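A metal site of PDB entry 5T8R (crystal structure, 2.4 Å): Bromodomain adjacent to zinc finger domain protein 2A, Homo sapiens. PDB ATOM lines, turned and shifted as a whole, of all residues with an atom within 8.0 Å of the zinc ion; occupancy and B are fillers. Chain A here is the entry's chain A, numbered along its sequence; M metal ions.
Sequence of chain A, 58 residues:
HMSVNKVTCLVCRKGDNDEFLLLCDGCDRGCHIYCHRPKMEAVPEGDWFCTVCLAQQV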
ATOM      1  N   THR A   8       4.963   6.252  -8.270  1.00  0.00           N
ATOM      2  CA  THR A   8       5.218   7.692  -8.106  1.00  0.00           C
ATOM      3  C   THR A   8       4.360   8.544  -9.036  1.00  0.00           C
ATOM      4  O   THR A   8       3.859   8.092 -10.075  1.00  0.00           O
ATOM      5  CB  THR A   8       6.715   8.073  -8.270  1.00  0.00           C
ATOM      6  OG1 THR A   8       7.151   7.803  -9.611  1.00  0.00           O
ATOM      7  CG2 THR A   8       7.594   7.314  -7.278  1.00  0.00           C
ATOM      8  N   CYS A   9       4.227   9.813  -8.652  1.00  0.00           N
ATOM      9  CA  CYS A   9       3.474  10.803  -9.421  1.00  0.00           C
ATOM     10  C   CYS A   9       4.222  11.263 -10.689  1.00  0.00           C
ATOM     11  O   CYS A   9       5.399  11.607 -10.639  1.00  0.00           O
ATOM     12  CB  CYS A   9       3.176  11.983  -8.500  1.00  0.00           C
ATOM     13  SG  CYS A   9       2.294  13.410  -9.183  1.00  0.00           S
ATOM     14  N   LEU A  10       3.526  11.284 -11.816  1.00  0.00           N
ATOM     15  CA  LEU A  10       4.110  11.778 -13.079  1.00  0.00           C
ATOM     16  C   LEU A  10       4.556  13.238 -13.054  1.00  0.00           C
ATOM     17  O   LEU A  10       5.488  13.597 -13.772  1.00  0.00           O
ATOM     18  CB  LEU A  10       3.128  11.586 -14.242  1.00  0.00           C
ATOM     19  CG  LEU A  10       2.978  10.174 -14.787  1.00  0.00           C
ATOM     20  CD1 LEU A  10       1.835  10.148 -15.806  1.00  0.00           C
ATOM     21  CD2 LEU A  10       4.263   9.679 -15.428  1.00  0.00           C
ATOM     22  N   VAL A  11       3.910  14.056 -12.241  1.00  0.00           N
ATOM     23  CA  VAL A  11       4.161  15.491 -12.166  1.00  0.00           C
ATOM     24  C   VAL A  11       5.324  15.839 -11.245  1.00  0.00           C
ATOM     25  O   VAL A  11       6.250  16.513 -11.650  1.00  0.00           O
ATOM     26  CB  VAL A  11       2.879  16.231 -11.668  1.00  0.00           C
ATOM     27  CG1 VAL A  11       3.110  17.730 -11.617  1.00  0.00           C
ATOM     28  CG2 VAL A  11       1.680  15.896 -12.545  1.00  0.00           C
ATOM     29  N   CYS A  12       5.252  15.421  -9.985  1.00  0.00           N
ATOM     30  CA  CYS A  12       6.222  15.790  -8.960  1.00  0.00           C
ATOM     31  C   CYS A  12       7.233  14.683  -8.647  1.00  0.00           C
ATOM     32  O   CYS A  12       8.239  14.954  -7.984  1.00  0.00           O
ATOM     33  CB  CYS A  12       5.506  16.233  -7.678  1.00  0.00           C
ATOM     34  SG  CYS A  12       4.741  14.893  -6.748  1.00  0.00           S
ATOM     35  N   ARG A  13       6.972  13.459  -9.111  1.00  0.00           N
ATOM     36  CA  ARG A  13       7.917  12.317  -8.960  1.00  0.00           C
ATOM     37  C   ARG A  13       8.099  11.783  -7.522  1.00  0.00           C
ATOM     38  O   ARG A  13       8.934  10.932  -7.288  1.00  0.00           O
ATOM     39  CB  ARG A  13       9.311  12.623  -9.579  1.00  0.00           C
ATOM     40  CG  ARG A  13       9.331  13.202 -10.991  1.00  0.00           C
ATOM     41  CD  ARG A  13       8.587  12.329 -11.981  1.00  0.00           C
ATOM     42  NE  ARG A  13       9.175  12.354 -13.339  1.00  0.00           N
ATOM     43  CZ  ARG A  13       8.689  11.704 -14.406  1.00  0.00           C
ATOM     44  NH1 ARG A  13       9.316  11.796 -15.594  1.00  0.00           N
ATOM     45  NH2 ARG A  13       7.571  10.965 -14.326  1.00  0.00           N
ATOM     46  N   LYS A  14       7.307  12.269  -6.565  1.00  0.00           N
ATOM     47  CA  LYS A  14       7.316  11.753  -5.206  1.00  0.00           C
ATOM     48  C   LYS A  14       6.206  10.685  -5.068  1.00  0.00           C
ATOM     49  O   LYS A  14       5.175  10.736  -5.734  1.00  0.00           O
ATOM     50  CB  LYS A  14       7.097  12.880  -4.198  1.00  0.00           C
ATOM     51  CG  LYS A  14       8.035  14.076  -4.397  1.00  0.00           C
ATOM     52  CD  LYS A  14       7.927  15.106  -3.282  1.00  0.00           C
ATOM     53  CE  LYS A  14       8.945  16.228  -3.449  1.00  0.00           C
ATOM     54  NZ  LYS A  14       9.196  16.995  -2.195  1.00  0.00           N
ATOM     55  N   GLY A  15       6.464   9.708  -4.213  1.00  0.00           N
ATOM     56  CA  GLY A  15       5.506   8.646  -3.905  1.00  0.00           C
ATOM     57  C   GLY A  15       4.779   8.816  -2.570  1.00  0.00           C
ATOM     58  O   GLY A  15       4.188   7.848  -2.070  1.00  0.00           O
ATOM     59  N   ASP A  16       4.833  10.017  -1.999  1.00  0.00           N
ATOM     60  CA  ASP A  16       4.193  10.289  -0.696  1.00  0.00           C
ATOM     61  C   ASP A  16       2.697  10.615  -0.859  1.00  0.00           C
ATOM     62  O   ASP A  16       2.212  10.736  -1.990  1.00  0.00           O
ATOM     63  CB  ASP A  16       4.953  11.363   0.096  1.00  0.00           C
ATOM     64  CG  ASP A  16       4.962  12.733  -0.593  1.00  0.00           C
ATOM     65  OD1 ASP A  16       4.393  12.883  -1.699  1.00  0.00           O
ATOM     66  OD2 ASP A  16       5.558  13.663   0.000  1.00  0.00           O
ATOM     67  N   ASN A  17       2.006  10.726   0.266  1.00  0.00           N
ATOM     68  CA  ASN A  17       0.562  10.978   0.306  1.00  0.00           C
ATOM     69  C   ASN A  17      -0.250  10.015  -0.538  1.00  0.00           C
ATOM     70  O   ASN A  17      -0.973  10.426  -1.447  1.00  0.00           O
ATOM     71  CB  ASN A  17       0.275  12.443  -0.042  1.00  0.00           C
ATOM     72  CG  ASN A  17       0.755  13.398   1.034  1.00  0.00           C
ATOM     73  OD1 ASN A  17       0.624  13.117   2.221  1.00  0.00           O
ATOM     74  ND2 ASN A  17       1.308  14.519   0.631  1.00  0.00           N
ATOM     75  N   PHE A  20      -3.938  10.485  -1.718  1.00  0.00           N
ATOM     76  CA  PHE A  20      -4.229  11.373  -2.843  1.00  0.00           C
ATOM     77  C   PHE A  20      -3.616  10.896  -4.172  1.00  0.00           C
ATOM     78  O   PHE A  20      -3.721  11.597  -5.176  1.00  0.00           O
ATOM     79  CB  PHE A  20      -3.706  12.774  -2.523  1.00  0.00           C
ATOM     80  CG  PHE A  20      -4.280  13.370  -1.278  1.00  0.00           C
ATOM     81  CD1 PHE A  20      -3.736  13.079  -0.022  1.00  0.00           C
ATOM     82  CD2 PHE A  20      -5.358  14.252  -1.331  1.00  0.00           C
ATOM     83  CE1 PHE A  20      -4.265  13.641   1.145  1.00  0.00           C
ATOM     84  CE2 PHE A  20      -5.888  14.818  -0.173  1.00  0.00           C
ATOM     85  CZ  PHE A  20      -5.340  14.507   1.062  1.00  0.00           C
ATOM     86  N   LEU A  21      -2.986   9.724  -4.213  1.00  0.00           N
ATOM     87  CA  LEU A  21      -2.138   9.358  -5.334  1.00  0.00           C
ATOM     88  C   LEU A  21      -2.916   8.420  -6.249  1.00  0.00           C
ATOM     89  O   LEU A  21      -2.974   7.225  -6.017  1.00  0.00           O
ATOM     90  CB  LEU A  21      -0.808   8.744  -4.848  1.00  0.00           C
ATOM     91  CG  LEU A  21       0.305   8.371  -5.864  1.00  0.00           C
ATOM     92  CD1 LEU A  21       0.375   9.266  -7.092  1.00  0.00           C
ATOM     93  CD2 LEU A  21       1.662   8.351  -5.184  1.00  0.00           C
ATOM     94  N   GLY A  30       1.145   6.954 -11.969  1.00  0.00           N
ATOM     95  CA  GLY A  30       0.337   7.614 -10.951  1.00  0.00           C
ATOM     96  C   GLY A  30       0.326   9.101 -11.038  1.00  0.00           C
ATOM     97  O   GLY A  30       1.161   9.685 -11.695  1.00  0.00           O
ATOM     98  N   CYS A  31      -0.644   9.723 -10.371  1.00  0.00           N
ATOM     99  CA  CYS A  31      -0.672  11.172 -10.207  1.00  0.00           C
ATOM    100  C   CYS A  31      -1.393  11.571  -8.900  1.00  0.00           C
ATOM    101  O   CYS A  31      -2.481  11.077  -8.611  1.00  0.00           O
ATOM    102  CB  CYS A  31      -1.374  11.816 -11.410  1.00  0.00           C
ATOM    103  SG  CYS A  31      -1.247  13.621 -11.548  1.00  0.00           S
ATOM    104  N   HIS A  32      -0.777  12.456  -8.109  1.00  0.00           N
ATOM    105  CA  HIS A  32      -1.490  13.094  -7.015  1.00  0.00           C
ATOM    106  C   HIS A  32      -2.628  13.934  -7.556  1.00  0.00           C
ATOM    107  O   HIS A  32      -2.408  14.733  -8.472  1.00  0.00           O
ATOM    108  CB  HIS A  32      -0.574  14.025  -6.233  1.00  0.00           C
ATOM    109  CG  HIS A  32       0.512  13.320  -5.511  1.00  0.00           C
ATOM    110  ND1 HIS A  32       1.842  13.517  -5.827  1.00  0.00           N
ATOM    111  CD2 HIS A  32       0.496  12.422  -4.503  1.00  0.00           C
ATOM    112  CE1 HIS A  32       2.587  12.762  -5.036  1.00  0.00           C
ATOM    113  NE2 HIS A  32       1.798  12.089  -4.228  1.00  0.00           N
ATOM    114  N   ILE A  33      -3.816  13.823  -6.976  1.00  0.00           N
ATOM    115  CA  ILE A  33      -4.942  14.666  -7.406  1.00  0.00           C
ATOM    116  C   ILE A  33      -4.614  16.163  -7.303  1.00  0.00           C
ATOM    117  O   ILE A  33      -5.038  16.953  -8.155  1.00  0.00           O
ATOM    118  CB  ILE A  33      -6.262  14.344  -6.650  1.00  0.00           C
ATOM    119  CG1 ILE A  33      -6.152  14.594  -5.150  1.00  0.00           C
ATOM    120  CG2 ILE A  33      -6.702  12.907  -6.899  1.00  0.00           C
ATOM    121  CD1 ILE A  33      -7.502  14.665  -4.507  1.00  0.00           C
ATOM    122  N   TYR A  34      -3.813  16.541  -6.306  1.00  0.00           N
ATOM    123  CA  TYR A  34      -3.390  17.935  -6.120  1.00  0.00           C
ATOM    124  C   TYR A  34      -2.311  18.403  -7.097  1.00  0.00           C
ATOM    125  O   TYR A  34      -2.057  19.591  -7.182  1.00  0.00           O
ATOM    126  CB  TYR A  34      -2.942  18.214  -4.664  1.00  0.00           C
ATOM    127  CG  TYR A  34      -1.838  17.329  -4.105  1.00  0.00           C
ATOM    128  CD1 TYR A  34      -0.499  17.550  -4.434  1.00  0.00           C
ATOM    129  CD2 TYR A  34      -2.129  16.292  -3.212  1.00  0.00           C
ATOM    130  CE1 TYR A  34       0.521  16.755  -3.910  1.00  0.00           C
ATOM    131  CE2 TYR A  34      -1.122  15.490  -2.679  1.00  0.00           C
ATOM    132  CZ  TYR A  34       0.209  15.712  -3.029  1.00  0.00           C
ATOM    133  OH  TYR A  34       1.230  14.913  -2.496  1.00  0.00           O
ATOM    134  N   CYS A  35      -1.655  17.487  -7.801  1.00  0.00           N
ATOM    135  CA  CYS A  35      -0.736  17.861  -8.866  1.00  0.00           C
ATOM    136  C   CYS A  35      -1.423  17.993 -10.254  1.00  0.00           C
ATOM    137  O   CYS A  35      -0.870  18.588 -11.177  1.00  0.00           O
ATOM    138  CB  CYS A  35       0.425  16.850  -8.929  1.00  0.00           C
ATOM    139  SG  CYS A  35       1.572  16.883  -7.530  1.00  0.00           S
ATOM    140  N   HIS A  36      -2.627  17.426 -10.393  1.00  0.00           N
ATOM    141  CA  HIS A  36      -3.358  17.408 -11.633  1.00  0.00           C
ATOM    142  C   HIS A  36      -3.836  18.820 -11.968  1.00  0.00           C
ATOM    143  O   HIS A  36      -4.220  19.565 -11.080  1.00  0.00           O
ATOM    144  CB  HIS A  36      -4.561  16.486 -11.515  1.00  0.00           C
ATOM    145  CG  HIS A  36      -5.160  16.059 -12.818  1.00  0.00           C
ATOM    146  ND1 HIS A  36      -6.096  16.827 -13.487  1.00  0.00           N
ATOM    147  CD2 HIS A  36      -4.968  14.953 -13.568  1.00  0.00           C
ATOM    148  CE1 HIS A  36      -6.453  16.200 -14.606  1.00  0.00           C
ATOM    149  NE2 HIS A  36      -5.781  15.068 -14.668  1.00  0.00           N
HETATM  150 ZN    ZN M   1       2.504  14.785  -7.331  1.00  0.00          ZN
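Four residues have an atom within 4 Å of the zinc ion: Cys 9, Cys 12, His 32 and Cys 35.
Along chain A the residues within 4 Å of the zinc ion span positions 9 to 35.
The nearest printed residue that does not touch the zinc ion is Tyr 34 (4.4 Å).
ND1 of His 32 binds the zinc ion (2.1 Å).
The zinc ion is bound by SG of Cys 35, 2.3 Å away.
SG of Cys 12 is bound to the zinc ion (2.3 Å).
The side-chain sulfur (SG) of Cys 9 binds the zinc ion (2.3 Å).
The zinc ion has four donor atoms within binding distance.
The side-chain hydroxyl of Tyr 34 sits close to a ring nitrogen (NE2) of His 32 (3.4 Å).
A ring nitrogen (NE2) of His 32 sits at hydrogen-bond distance from the backbone carbonyl oxygen (O) of Asp 16, at 2.6 Å.
The backbone NH (N) of Cys 9 lies within hydrogen-bond range of the backbone carbonyl oxygen (O) of Lys 14 (3.2 Å).
SG of Cys 9 lies close to N of Val 11, 3.5 Å away.
SG of Cys 12 lies close to N of Lys 14 (3.7 Å).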
